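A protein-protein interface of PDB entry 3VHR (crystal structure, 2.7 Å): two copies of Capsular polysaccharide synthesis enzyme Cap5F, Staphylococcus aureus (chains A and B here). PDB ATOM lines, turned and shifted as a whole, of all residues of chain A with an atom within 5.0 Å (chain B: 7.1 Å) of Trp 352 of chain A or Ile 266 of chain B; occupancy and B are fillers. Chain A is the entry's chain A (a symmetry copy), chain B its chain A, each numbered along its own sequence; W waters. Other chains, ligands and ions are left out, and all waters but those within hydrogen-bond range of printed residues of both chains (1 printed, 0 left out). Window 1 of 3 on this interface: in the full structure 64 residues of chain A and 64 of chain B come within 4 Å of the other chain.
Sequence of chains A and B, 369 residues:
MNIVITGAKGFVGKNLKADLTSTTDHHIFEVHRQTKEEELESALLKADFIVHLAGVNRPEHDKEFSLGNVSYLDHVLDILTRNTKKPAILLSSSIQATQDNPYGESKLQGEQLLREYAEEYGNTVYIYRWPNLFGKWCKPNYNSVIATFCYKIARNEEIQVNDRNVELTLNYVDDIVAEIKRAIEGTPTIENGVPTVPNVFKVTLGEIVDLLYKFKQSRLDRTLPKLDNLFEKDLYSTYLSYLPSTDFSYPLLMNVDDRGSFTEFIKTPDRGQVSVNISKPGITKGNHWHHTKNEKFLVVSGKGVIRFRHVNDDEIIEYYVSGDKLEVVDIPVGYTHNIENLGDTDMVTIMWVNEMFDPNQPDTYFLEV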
ATOM      1  N   ARG A 271       3.953 -18.617   5.454  1.00  0.00           N
ATOM      2  CA  ARG A 271       2.786 -17.731   5.429  1.00  0.00           C
ATOM      3  C   ARG A 271       2.976 -16.502   6.334  1.00  0.00           C
ATOM      4  O   ARG A 271       2.006 -15.888   6.778  1.00  0.00           O
ATOM      5  CB  ARG A 271       1.518 -18.500   5.838  1.00  0.00           C
ATOM      6  CG  ARG A 271       1.235 -19.744   5.012  1.00  0.00           C
ATOM      7  CD  ARG A 271       0.679 -19.438   3.635  1.00  0.00           C
ATOM      8  NE  ARG A 271       0.521 -20.683   2.902  1.00  0.00           N
ATOM      9  CZ  ARG A 271       0.250 -20.782   1.601  1.00  0.00           C
ATOM     10  NH1 ARG A 271       0.125 -21.985   1.043  1.00  0.00           N
ATOM     11  NH2 ARG A 271       0.104 -19.687   0.855  1.00  0.00           N
ATOM     12  N   GLY A 272       4.229 -16.160   6.619  1.00  0.00           N
ATOM     13  CA  GLY A 272       4.536 -14.986   7.417  1.00  0.00           C
ATOM     14  C   GLY A 272       4.174 -15.118   8.877  1.00  0.00           C
ATOM     15  O   GLY A 272       4.042 -16.227   9.391  1.00  0.00           O
ATOM     16  N   GLN A 273       4.028 -13.984   9.555  1.00  0.00           N
ATOM     17  CA  GLN A 273       3.742 -14.003  10.978  1.00  0.00           C
ATOM     18  C   GLN A 273       2.779 -12.918  11.416  1.00  0.00           C
ATOM     19  O   GLN A 273       2.681 -11.876  10.770  1.00  0.00           O
ATOM     20  CB  GLN A 273       5.039 -13.956  11.806  1.00  0.00           C
ATOM     21  CG  GLN A 273       5.841 -12.673  11.733  1.00  0.00           C
ATOM     22  CD  GLN A 273       6.812 -12.527  12.900  1.00  0.00           C
ATOM     23  OE1 GLN A 273       7.986 -12.889  12.793  1.00  0.00           O
ATOM     24  NE2 GLN A 273       6.321 -12.000  14.024  1.00  0.00           N
ATOM     25  N   VAL A 274       2.050 -13.178  12.500  1.00  0.00           N
ATOM     26  CA  VAL A 274       1.174 -12.158  13.071  1.00  0.00           C
ATOM     27  C   VAL A 274       1.553 -11.771  14.499  1.00  0.00           C
ATOM     28  O   VAL A 274       1.952 -12.612  15.297  1.00  0.00           O
ATOM     29  CB  VAL A 274      -0.354 -12.419  12.849  1.00  0.00           C
ATOM     30  CG1 VAL A 274      -0.630 -13.774  12.233  1.00  0.00           C
ATOM     31  CG2 VAL A 274      -1.172 -12.196  14.111  1.00  0.00           C
ATOM     32  N   ASN A 294       6.844  -6.636   3.699  1.00  0.00           N
ATOM     33  CA  ASN A 294       5.593  -5.899   3.674  1.00  0.00           C
ATOM     34  C   ASN A 294       4.617  -6.400   4.720  1.00  0.00           C
ATOM     35  O   ASN A 294       4.784  -7.495   5.272  1.00  0.00           O
ATOM     36  CB  ASN A 294       4.968  -5.880   2.293  1.00  0.00           C
ATOM     37  CG  ASN A 294       4.479  -7.230   1.857  1.00  0.00           C
ATOM     38  OD1 ASN A 294       5.128  -7.894   1.043  1.00  0.00           O
ATOM     39  ND2 ASN A 294       3.326  -7.640   2.369  1.00  0.00           N
ATOM     40  N   GLU A 295       3.615  -5.580   5.017  1.00  0.00           N
ATOM     41  CA  GLU A 295       2.741  -5.864   6.133  1.00  0.00           C
ATOM     42  C   GLU A 295       1.262  -5.692   5.806  1.00  0.00           C
ATOM     43  O   GLU A 295       0.893  -5.192   4.735  1.00  0.00           O
ATOM     44  CB  GLU A 295       3.160  -5.017   7.326  1.00  0.00           C
ATOM     45  CG  GLU A 295       4.605  -5.245   7.708  1.00  0.00           C
ATOM     46  CD  GLU A 295       5.329  -3.990   8.164  1.00  0.00           C
ATOM     47  OE1 GLU A 295       5.358  -2.959   7.441  1.00  0.00           O
ATOM     48  OE2 GLU A 295       5.901  -4.054   9.271  1.00  0.00           O
ATOM     49  N   LYS A 296       0.434  -6.163   6.731  1.00  0.00           N
ATOM     50  CA  LYS A 296      -0.994  -5.914   6.711  1.00  0.00           C
ATOM     51  C   LYS A 296      -1.388  -5.442   8.113  1.00  0.00           C
ATOM     52  O   LYS A 296      -1.168  -6.140   9.115  1.00  0.00           O
ATOM     53  CB  LYS A 296      -1.757  -7.178   6.328  1.00  0.00           C
ATOM     54  CG  LYS A 296      -1.508  -7.719   4.928  1.00  0.00           C
ATOM     55  CD  LYS A 296      -2.293  -8.999   4.733  1.00  0.00           C
ATOM     56  CE  LYS A 296      -2.264  -9.476   3.305  1.00  0.00           C
ATOM     57  NZ  LYS A 296      -3.026  -8.535   2.425  1.00  0.00           N
ATOM     58  N   ILE A 350      -3.405  -5.501  14.834  1.00  0.00           N
ATOM     59  CA  ILE A 350      -2.885  -6.815  14.429  1.00  0.00           C
ATOM     60  C   ILE A 350      -1.973  -6.619  13.229  1.00  0.00           C
ATOM     61  O   ILE A 350      -2.372  -6.013  12.238  1.00  0.00           O
ATOM     62  CB  ILE A 350      -4.013  -7.807  14.058  1.00  0.00           C
ATOM     63  CG1 ILE A 350      -5.036  -7.945  15.190  1.00  0.00           C
ATOM     64  CG2 ILE A 350      -3.448  -9.169  13.703  1.00  0.00           C
ATOM     65  CD1 ILE A 350      -4.438  -8.207  16.560  1.00  0.00           C
ATOM     66  N   MET A 351      -0.743  -7.106  13.319  1.00  0.00           N
ATOM     67  CA  MET A 351       0.216  -6.853  12.245  1.00  0.00           C
ATOM     68  C   MET A 351       0.656  -8.135  11.632  1.00  0.00           C
ATOM     69  O   MET A 351       1.256  -8.973  12.293  1.00  0.00           O
ATOM     70  CB  MET A 351       1.403  -6.051  12.758  1.00  0.00           C
ATOM     71  CG  MET A 351       0.918  -4.677  13.207  1.00  0.00           C
ATOM     72  SD  MET A 351       2.467  -3.566  13.721  1.00  0.00           S
ATOM     73  CE  MET A 351       1.767  -1.753  13.416  1.00  0.00           C
ATOM     74  N   TRP A 352       0.322  -8.317  10.364  1.00  0.00           N
ATOM     75  CA  TRP A 352       0.833  -9.452   9.617  1.00  0.00           C
ATOM     76  C   TRP A 352       2.050  -8.990   8.860  1.00  0.00           C
ATOM     77  O   TRP A 352       2.053  -7.884   8.324  1.00  0.00           O
ATOM     78  CB  TRP A 352      -0.236 -10.025   8.679  1.00  0.00           C
ATOM     79  CG  TRP A 352       0.299 -11.147   7.845  1.00  0.00           C
ATOM     80  CD1 TRP A 352       0.414 -12.481   8.200  1.00  0.00           C
ATOM     81  CD2 TRP A 352       0.881 -11.054   6.500  1.00  0.00           C
ATOM     82  NE1 TRP A 352       1.000 -13.202   7.192  1.00  0.00           N
ATOM     83  CE2 TRP A 352       1.305 -12.407   6.146  1.00  0.00           C
ATOM     84  CE3 TRP A 352       1.098 -10.016   5.593  1.00  0.00           C
ATOM     85  CZ2 TRP A 352       1.896 -12.694   4.928  1.00  0.00           C
ATOM     86  CZ3 TRP A 352       1.697 -10.318   4.366  1.00  0.00           C
ATOM     87  CH2 TRP A 352       2.087 -11.629   4.044  1.00  0.00           C
ATOM     88  N   VAL A 353       3.098  -9.802   8.829  1.00  0.00           N
ATOM     89  CA  VAL A 353       4.304  -9.461   8.071  1.00  0.00           C
ATOM     90  C   VAL A 353       4.732 -10.665   7.243  1.00  0.00           C
ATOM     91  O   VAL A 353       4.563 -11.796   7.679  1.00  0.00           O
ATOM     92  CB  VAL A 353       5.450  -8.927   8.983  1.00  0.00           C
ATOM     93  CG1 VAL A 353       5.830  -9.940  10.039  1.00  0.00           C
ATOM     94  CG2 VAL A 353       6.669  -8.555   8.162  1.00  0.00           C
ATOM     95  N   ASN A 354       5.272 -10.412   6.052  1.00  0.00           N
ATOM     96  CA  ASN A 354       5.543 -11.457   5.042  1.00  0.00           C
ATOM     97  C   ASN A 354       6.752 -12.358   5.299  1.00  0.00           C
ATOM     98  O   ASN A 354       7.102 -13.191   4.468  1.00  0.00           O
ATOM     99  CB  ASN A 354       5.669 -10.824   3.645  1.00  0.00           C
ATOM    100  CG  ASN A 354       6.996 -10.081   3.431  1.00  0.00           C
ATOM    101  OD1 ASN A 354       7.545  -9.471   4.340  1.00  0.00           O
ATOM    102  ND2 ASN A 354       7.498 -10.124   2.207  1.00  0.00           N
ATOM    103  N   ASP B 221     -10.564 -13.248  -0.926  1.00  0.00           N
ATOM    104  CA  ASP B 221     -10.673 -14.530  -0.232  1.00  0.00           C
ATOM    105  C   ASP B 221      -9.775 -14.676   1.001  1.00  0.00           C
ATOM    106  O   ASP B 221      -9.767 -15.728   1.637  1.00  0.00           O
ATOM    107  CB  ASP B 221     -10.505 -15.707  -1.214  1.00  0.00           C
ATOM    108  CG  ASP B 221      -9.100 -15.801  -1.806  1.00  0.00           C
ATOM    109  OD1 ASP B 221      -8.159 -15.173  -1.267  1.00  0.00           O
ATOM    110  OD2 ASP B 221      -8.934 -16.517  -2.813  1.00  0.00           O
ATOM    111  N   ARG B 222      -9.048 -13.610   1.339  1.00  0.00           N
ATOM    112  CA  ARG B 222      -8.211 -13.516   2.551  1.00  0.00           C
ATOM    113  C   ARG B 222      -7.061 -14.522   2.587  1.00  0.00           C
ATOM    114  O   ARG B 222      -6.493 -14.780   3.647  1.00  0.00           O
ATOM    115  CB  ARG B 222      -9.028 -13.664   3.850  1.00  0.00           C
ATOM    116  CG  ARG B 222     -10.486 -13.271   3.802  1.00  0.00           C
ATOM    117  CD  ARG B 222     -10.655 -11.776   3.746  1.00  0.00           C
ATOM    118  NE  ARG B 222     -12.071 -11.446   3.644  1.00  0.00           N
ATOM    119  CZ  ARG B 222     -12.543 -10.365   3.033  1.00  0.00           C
ATOM    120  NH1 ARG B 222     -11.713  -9.501   2.453  1.00  0.00           N
ATOM    121  NH2 ARG B 222     -13.847 -10.151   2.995  1.00  0.00           N
ATOM    122  N   THR B 223      -6.726 -15.106   1.445  1.00  0.00           N
ATOM    123  CA  THR B 223      -5.607 -16.032   1.388  1.00  0.00           C
ATOM    124  C   THR B 223      -4.292 -15.272   1.245  1.00  0.00           C
ATOM    125  O   THR B 223      -4.273 -14.088   0.917  1.00  0.00           O
ATOM    126  CB  THR B 223      -5.762 -17.042   0.247  1.00  0.00           C
ATOM    127  OG1 THR B 223      -5.756 -16.347  -1.005  1.00  0.00           O
ATOM    128  CG2 THR B 223      -7.057 -17.843   0.405  1.00  0.00           C
ATOM    129  N   LEU B 224      -3.194 -15.965   1.504  1.00  0.00           N
ATOM    130  CA  LEU B 224      -1.856 -15.385   1.487  1.00  0.00           C
ATOM    131  C   LEU B 224      -1.023 -16.097   0.418  1.00  0.00           C
ATOM    132  O   LEU B 224      -1.393 -17.203  -0.013  1.00  0.00           O
ATOM    133  CB  LEU B 224      -1.215 -15.569   2.863  1.00  0.00           C
ATOM    134  CG  LEU B 224      -1.213 -14.484   3.957  1.00  0.00           C
ATOM    135  CD1 LEU B 224      -2.059 -13.258   3.655  1.00  0.00           C
ATOM    136  CD2 LEU B 224      -1.596 -15.116   5.278  1.00  0.00           C
ATOM    137  N   PRO B 225       0.094 -15.474  -0.027  1.00  0.00           N
ATOM    138  CA  PRO B 225       0.984 -16.101  -1.020  1.00  0.00           C
ATOM    139  C   PRO B 225       1.848 -17.181  -0.377  1.00  0.00           C
ATOM    140  O   PRO B 225       1.896 -17.250   0.840  1.00  0.00           O
ATOM    141  CB  PRO B 225       1.871 -14.946  -1.493  1.00  0.00           C
ATOM    142  CG  PRO B 225       1.417 -13.719  -0.773  1.00  0.00           C
ATOM    143  CD  PRO B 225       0.578 -14.147   0.388  1.00  0.00           C
ATOM    144  N   LEU B 227       5.033 -17.823   0.733  1.00  0.00           N
ATOM    145  CA  LEU B 227       6.206 -16.995   1.022  1.00  0.00           C
ATOM    146  C   LEU B 227       7.569 -17.727   1.096  1.00  0.00           C
ATOM    147  O   LEU B 227       8.609 -17.084   1.190  1.00  0.00           O
ATOM    148  CB  LEU B 227       5.966 -16.139   2.272  1.00  0.00           C
ATOM    149  CG  LEU B 227       5.226 -14.813   2.104  1.00  0.00           C
ATOM    150  CD1 LEU B 227       5.329 -14.283   0.682  1.00  0.00           C
ATOM    151  CD2 LEU B 227       3.778 -14.903   2.506  1.00  0.00           C
ATOM    152  N   TYR B 236       5.429 -10.772  -5.117  1.00  0.00           N
ATOM    153  CA  TYR B 236       4.351 -10.212  -4.304  1.00  0.00           C
ATOM    154  C   TYR B 236       4.716  -8.820  -3.812  1.00  0.00           C
ATOM    155  O   TYR B 236       3.915  -7.883  -3.898  1.00  0.00           O
ATOM    156  CB  TYR B 236       3.984 -11.145  -3.132  1.00  0.00           C
ATOM    157  CG  TYR B 236       2.858 -10.620  -2.251  1.00  0.00           C
ATOM    158  CD1 TYR B 236       1.566 -10.491  -2.748  1.00  0.00           C
ATOM    159  CD2 TYR B 236       3.084 -10.254  -0.923  1.00  0.00           C
ATOM    160  CE1 TYR B 236       0.532 -10.009  -1.952  1.00  0.00           C
ATOM    161  CE2 TYR B 236       2.057  -9.767  -0.123  1.00  0.00           C
ATOM    162  CZ  TYR B 236       0.787  -9.651  -0.645  1.00  0.00           C
ATOM    163  OH  TYR B 236      -0.252  -9.178   0.112  1.00  0.00           O
ATOM    164  N   LEU B 240       2.810  -5.194  -4.967  1.00  0.00           N
ATOM    165  CA  LEU B 240       2.249  -4.258  -4.009  1.00  0.00           C
ATOM    166  C   LEU B 240       2.701  -2.853  -4.325  1.00  0.00           C
ATOM    167  O   LEU B 240       1.911  -1.924  -4.240  1.00  0.00           O
ATOM    168  CB  LEU B 240       2.646  -4.630  -2.586  1.00  0.00           C
ATOM    169  CG  LEU B 240       1.669  -5.335  -1.642  1.00  0.00           C
ATOM    170  CD1 LEU B 240       0.609  -6.186  -2.327  1.00  0.00           C
ATOM    171  CD2 LEU B 240       2.487  -6.142  -0.646  1.00  0.00           C
ATOM    172  N   TYR B 250      -8.454  -2.653   2.046  1.00  0.00           N
ATOM    173  CA  TYR B 250      -9.608  -3.364   1.525  1.00  0.00           C
ATOM    174  C   TYR B 250     -10.519  -3.734   2.663  1.00  0.00           C
ATOM    175  O   TYR B 250     -10.047  -4.046   3.743  1.00  0.00           O
ATOM    176  CB  TYR B 250      -9.193  -4.605   0.722  1.00  0.00           C
ATOM    177  CG  TYR B 250      -8.209  -5.544   1.401  1.00  0.00           C
ATOM    178  CD1 TYR B 250      -6.843  -5.243   1.446  1.00  0.00           C
ATOM    179  CD2 TYR B 250      -8.640  -6.748   1.965  1.00  0.00           C
ATOM    180  CE1 TYR B 250      -5.942  -6.103   2.033  1.00  0.00           C
ATOM    181  CE2 TYR B 250      -7.747  -7.618   2.558  1.00  0.00           C
ATOM    182  CZ  TYR B 250      -6.395  -7.293   2.589  1.00  0.00           C
ATOM    183  OH  TYR B 250      -5.485  -8.153   3.196  1.00  0.00           O
ATOM    184  N   LEU B 252     -13.000  -5.763   5.124  1.00  0.00           N
ATOM    185  CA  LEU B 252     -13.213  -7.119   5.599  1.00  0.00           C
ATOM    186  C   LEU B 252     -14.709  -7.315   5.823  1.00  0.00           C
ATOM    187  O   LEU B 252     -15.418  -6.348   6.075  1.00  0.00           O
ATOM    188  CB  LEU B 252     -12.474  -7.301   6.920  1.00  0.00           C
ATOM    189  CG  LEU B 252     -11.245  -8.193   7.041  1.00  0.00           C
ATOM    190  CD1 LEU B 252     -10.357  -8.194   5.815  1.00  0.00           C
ATOM    191  CD2 LEU B 252     -10.467  -7.798   8.282  1.00  0.00           C
ATOM    192  N   THR B 263     -15.204 -11.605  12.354  1.00  0.00           N
ATOM    193  CA  THR B 263     -14.607 -11.182  11.090  1.00  0.00           C
ATOM    194  C   THR B 263     -13.406 -12.051  10.768  1.00  0.00           C
ATOM    195  O   THR B 263     -12.508 -12.188  11.606  1.00  0.00           O
ATOM    196  CB  THR B 263     -14.104  -9.729  11.205  1.00  0.00           C
ATOM    197  OG1 THR B 263     -15.050  -8.937  11.941  1.00  0.00           O
ATOM    198  CG2 THR B 263     -13.869  -9.119   9.840  1.00  0.00           C
ATOM    199  N   GLU B 264     -13.392 -12.639   9.567  1.00  0.00           N
ATOM    200  CA  GLU B 264     -12.197 -13.329   9.044  1.00  0.00           C
ATOM    201  C   GLU B 264     -11.152 -12.327   8.560  1.00  0.00           C
ATOM    202  O   GLU B 264     -11.499 -11.283   8.028  1.00  0.00           O
ATOM    203  CB  GLU B 264     -12.574 -14.284   7.921  1.00  0.00           C
ATOM    204  CG  GLU B 264     -13.256 -15.552   8.418  1.00  0.00           C
ATOM    205  CD  GLU B 264     -13.998 -16.302   7.321  1.00  0.00           C
ATOM    206  OE1 GLU B 264     -14.107 -15.777   6.189  1.00  0.00           O
ATOM    207  OE2 GLU B 264     -14.477 -17.423   7.588  1.00  0.00           O
ATOM    208  N   PHE B 265      -9.877 -12.650   8.752  1.00  0.00           N
ATOM    209  CA  PHE B 265      -8.765 -11.757   8.404  1.00  0.00           C
ATOM    210  C   PHE B 265      -7.823 -12.405   7.369  1.00  0.00           C
ATOM    211  O   PHE B 265      -7.725 -11.924   6.227  1.00  0.00           O
ATOM    212  CB  PHE B 265      -8.024 -11.349   9.683  1.00  0.00           C
ATOM    213  CG  PHE B 265      -6.701 -10.664   9.457  1.00  0.00           C
ATOM    214  CD1 PHE B 265      -6.512  -9.759   8.403  1.00  0.00           C
ATOM    215  CD2 PHE B 265      -5.636 -10.882  10.337  1.00  0.00           C
ATOM    216  CE1 PHE B 265      -5.283  -9.122   8.217  1.00  0.00           C
ATOM    217  CE2 PHE B 265      -4.411 -10.234  10.149  1.00  0.00           C
ATOM    218  CZ  PHE B 265      -4.236  -9.351   9.090  1.00  0.00           C
ATOM    219  N   ILE B 266      -7.136 -13.480   7.772  1.00  0.00           N
ATOM    220  CA  ILE B 266      -6.306 -14.277   6.853  1.00  0.00           C
ATOM    221  C   ILE B 266      -6.633 -15.786   6.911  1.00  0.00           C
ATOM    222  O   ILE B 266      -6.918 -16.327   7.984  1.00  0.00           O
ATOM    223  CB  ILE B 266      -4.776 -14.017   7.019  1.00  0.00           C
ATOM    224  CG1 ILE B 266      -4.255 -14.469   8.381  1.00  0.00           C
ATOM    225  CG2 ILE B 266      -4.409 -12.556   6.740  1.00  0.00           C
ATOM    226  CD1 ILE B 266      -2.901 -13.902   8.727  1.00  0.00           C
ATOM    227  N   LYS B 267      -6.614 -16.437   5.743  1.00  0.00           N
ATOM    228  CA  LYS B 267      -6.868 -17.891   5.599  1.00  0.00           C
ATOM    229  C   LYS B 267      -5.714 -18.584   4.867  1.00  0.00           C
ATOM    230  O   LYS B 267      -5.130 -18.019   3.936  1.00  0.00           O
ATOM    231  CB  LYS B 267      -8.172 -18.161   4.824  1.00  0.00           C
ATOM    232  CG  LYS B 267      -9.313 -17.187   5.102  1.00  0.00           C
ATOM    233  CD  LYS B 267     -10.673 -17.860   5.113  1.00  0.00           C
ATOM    234  CE  LYS B 267     -11.467 -17.554   3.852  1.00  0.00           C
ATOM    235  NZ  LYS B 267     -12.928 -17.676   4.119  1.00  0.00           N
ATOM    236  N   THR B 268      -5.371 -19.801   5.281  1.00  0.00           N
ATOM    237  CA  THR B 268      -4.337 -20.581   4.567  1.00  0.00           C
ATOM    238  C   THR B 268      -4.652 -22.060   4.608  1.00  0.00           C
ATOM    239  O   THR B 268      -5.180 -22.541   5.609  1.00  0.00           O
ATOM    240  CB  THR B 268      -2.914 -20.395   5.140  1.00  0.00           C
ATOM    241  OG1 THR B 268      -2.830 -21.021   6.423  1.00  0.00           O
ATOM    242  CG2 THR B 268      -2.545 -18.935   5.265  1.00  0.00           C
ATOM    243  N   GLY B 272      -3.563 -22.804   8.843  1.00  0.00           N
ATOM    244  CA  GLY B 272      -4.816 -22.397   9.454  1.00  0.00           C
ATOM    245  C   GLY B 272      -5.225 -20.976   9.142  1.00  0.00           C
ATOM    246  O   GLY B 272      -4.774 -20.400   8.155  1.00  0.00           O
ATOM    247  N   GLN B 273      -6.093 -20.415   9.976  1.00  0.00           N
ATOM    248  CA  GLN B 273      -6.597 -19.076   9.729  1.00  0.00           C
ATOM    249  C   GLN B 273      -6.775 -18.254  10.991  1.00  0.00           C
ATOM    250  O   GLN B 273      -6.968 -18.808  12.071  1.00  0.00           O
ATOM    251  CB  GLN B 273      -7.899 -19.114   8.909  1.00  0.00           C
ATOM    252  CG  GLN B 273      -9.112 -19.711   9.593  1.00  0.00           C
ATOM    253  CD  GLN B 273     -10.419 -19.295   8.927  1.00  0.00           C
ATOM    254  OE1 GLN B 273     -10.948 -20.010   8.074  1.00  0.00           O
ATOM    255  NE2 GLN B 273     -10.941 -18.128   9.313  1.00  0.00           N
ATOM    256  N   VAL B 274      -6.681 -16.932  10.853  1.00  0.00           N
ATOM    257  CA  VAL B 274      -6.946 -16.045  11.982  1.00  0.00           C
ATOM    258  C   VAL B 274      -8.122 -15.101  11.740  1.00  0.00           C
ATOM    259  O   VAL B 274      -8.316 -14.602  10.638  1.00  0.00           O
ATOM    260  CB  VAL B 274      -5.671 -15.361  12.581  1.00  0.00           C
ATOM    261  CG1 VAL B 274      -4.429 -15.622  11.757  1.00  0.00           C
ATOM    262  CG2 VAL B 274      -5.874 -13.877  12.840  1.00  0.00           C
ATOM    263  N   SER B 275      -8.917 -14.906  12.787  1.00  0.00           N
ATOM    264  CA  SER B 275     -10.134 -14.114  12.724  1.00  0.00           C
ATOM    265  C   SER B 275     -10.271 -13.264  13.979  1.00  0.00           C
ATOM    266  O   SER B 275      -9.522 -13.437  14.950  1.00  0.00           O
ATOM    267  CB  SER B 275     -11.339 -15.036  12.607  1.00  0.00           C
ATOM    268  OG  SER B 275     -11.188 -15.897  11.502  1.00  0.00           O
ATOM    269  N   MET B 351      -8.598 -15.131  17.051  1.00  0.00           N
ATOM    270  CA  MET B 351      -8.847 -16.572  17.066  1.00  0.00           C
ATOM    271  C   MET B 351      -8.124 -17.233  15.947  1.00  0.00           C
ATOM    272  O   MET B 351      -8.386 -16.960  14.783  1.00  0.00           O
ATOM    273  CB  MET B 351     -10.339 -16.864  17.009  1.00  0.00           C
ATOM    274  CG  MET B 351     -11.001 -16.319  18.269  1.00  0.00           C
ATOM    275  SD  MET B 351     -12.908 -16.833  18.287  1.00  0.00           S
ATOM    276  CE  MET B 351     -13.297 -16.826  20.216  1.00  0.00           C
ATOM    277  N   TRP B 352      -7.171 -18.085  16.294  1.00  0.00           N
ATOM    278  CA  TRP B 352      -6.512 -18.908  15.296  1.00  0.00           C
ATOM    279  C   TRP B 352      -7.205 -20.244  15.275  1.00  0.00           C
ATOM    280  O   TRP B 352      -7.556 -20.768  16.329  1.00  0.00           O
ATOM    281  CB  TRP B 352      -5.014 -19.050  15.597  1.00  0.00           C
ATOM    282  CG  TRP B 352      -4.335 -19.958  14.621  1.00  0.00           C
ATOM    283  CD1 TRP B 352      -3.846 -19.634  13.366  1.00  0.00           C
ATOM    284  CD2 TRP B 352      -4.108 -21.402  14.762  1.00  0.00           C
ATOM    285  NE1 TRP B 352      -3.336 -20.744  12.743  1.00  0.00           N
ATOM    286  CE2 TRP B 352      -3.463 -21.836  13.524  1.00  0.00           C
ATOM    287  CE3 TRP B 352      -4.381 -22.348  15.752  1.00  0.00           C
ATOM    288  CZ2 TRP B 352      -3.095 -23.153  13.312  1.00  0.00           C
ATOM    289  CZ3 TRP B 352      -4.005 -23.676  15.526  1.00  0.00           C
ATOM    290  CH2 TRP B 352      -3.376 -24.067  14.332  1.00  0.00           C
ATOM    291  N   MET B 356      -9.504 -24.139   7.603  1.00  0.00           N
ATOM    292  CA  MET B 356     -10.496 -23.226   7.084  1.00  0.00           C
ATOM    293  C   MET B 356     -11.819 -23.856   7.351  1.00  0.00           C
ATOM    294  O   MET B 356     -11.964 -25.072   7.262  1.00  0.00           O
ATOM    295  CB  MET B 356     -10.253 -23.006   5.609  1.00  0.00           C
ATOM    296  CG  MET B 356      -9.209 -21.903   5.503  1.00  0.00           C
ATOM    297  SD  MET B 356      -8.480 -21.965   3.680  1.00  0.00           S
ATOM    298  CE  MET B 356     -10.179 -22.114   2.655  1.00  0.00           C
HETATM  299  O   HOH W   1       0.295  -7.668   2.206  1.00  0.00           O
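Thr 268 of chain B touches Arg 271 of chain A.
Tyr 236 of chain B touches Asn 294 of chain A (CE2 to ND2, 3.5 Å).
Asn 294 of chain A touches Leu 240 of chain B (CG to CD2, 3.4 Å).
Lys 296 of chain A touches Leu 224 of chain B.
OH of Tyr 236 of chain B touches NZ of Lys 296 of chain A (3.7 Å).
Ile 350 of chain A touches Phe 265 of chain B.
Leu 224 of chain B touches Trp 352 of chain A (CG to CZ2, 3.7 Å).
Trp 352 of chain A touches Leu 227 of chain B.
Water W1 lies within hydrogen-bond range of OH of Tyr 236 of chain B (2.6 Å), ND2 of Asn 294 of chain A (3.0 Å) and NZ of Lys 296 of chain A (3.4 Å).
Val 274 of chain A touches none of the printed residues of chain B.
Of the printed residues of chain B, Asn 294 of chain A touches Tyr 236 and Leu 240.
Trp 352 of chain A touches just these residues of chain B: Leu 224, Leu 227 and Ile 266.
Printed residues of chain A within 4 Å of Leu 227 of chain B: Trp 352 (3.8 Å) and Asn 354 (3.4 Å).
Of chain A, only Trp 352 (3.6 Å) comes within 4 Å of Ile 266 of chain B.
The nearest residue of chain B that does not touch Trp 352 of chain A is Phe 265 of chain B (4.1 Å).
The nearest printed residue of chain B that does not touch Arg 271 of chain A is Leu 227 of chain B (4.2 Å).
O of Val 274 of chain B is in hydrogen-bond range of N of Phe 265 of chain B, 3.1 Å away.
The backbone NH (N) of Val 274 of chain B is in hydrogen-bond range of the backbone carbonyl oxygen (O) of Ile 266 of chain B (2.9 Å).
OD1 of Asn 354 of chain A sits at hydrogen-bond distance from N of Asn 294 of chain A, 3.0 Å away.
The backbone NH of Lys 296 of chain A is in hydrogen-bond range of the backbone carbonyl oxygen of Trp 352 of chain A, at 2.8 Å.
Of the 23 printed residues of chain B, 9 touch a printed residue of chain A.
Printed residues of chain B that touch a printed residue of chain A: Leu 224, Pro 225, Leu 227, Tyr 236, Leu 240, Tyr 250, Phe 265, Ile 266 and Thr 268.
Hydrophobic or aromatic side chains of chain B within 4 Å of the printed part of chain A: Leu 224, Leu 227, Tyr 236, Leu 240, Tyr 250, Phe 265 and Ile 266.
Of the 12 printed residues of chain A, 6 touch a printed residue of chain B.
Printed residues of chain A that touch a printed residue of chain B: Arg 271, Asn 294, Lys 296, Ile 350, Trp 352 and Asn 354.
Hydrophobic or aromatic side chains of chain A that line the printed part of chain B: Ile 350 and Trp 352.
Along chain A the printed residues that touch a printed residue of chain B span positions 271 to 354.
Among the printed residues, 13 pairs touch across the chains.
The guanidinium group of Arg 271 of chain A lies within hydrogen-bond range of the backbone carbonyl oxygen of Leu 224 of chain B, 3.0 Å away.
O of Pro 225 of chain B sits at hydrogen-bond distance from NH2 of Arg 271 of chain A (3.0 Å).
The side-chain amino group of Lys 296 of chain A lies within hydrogen-bond range of the side-chain hydroxyl of Tyr 250 of chain B.
Positions printed for both chains: 272, 273, 274, 351 and 352.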
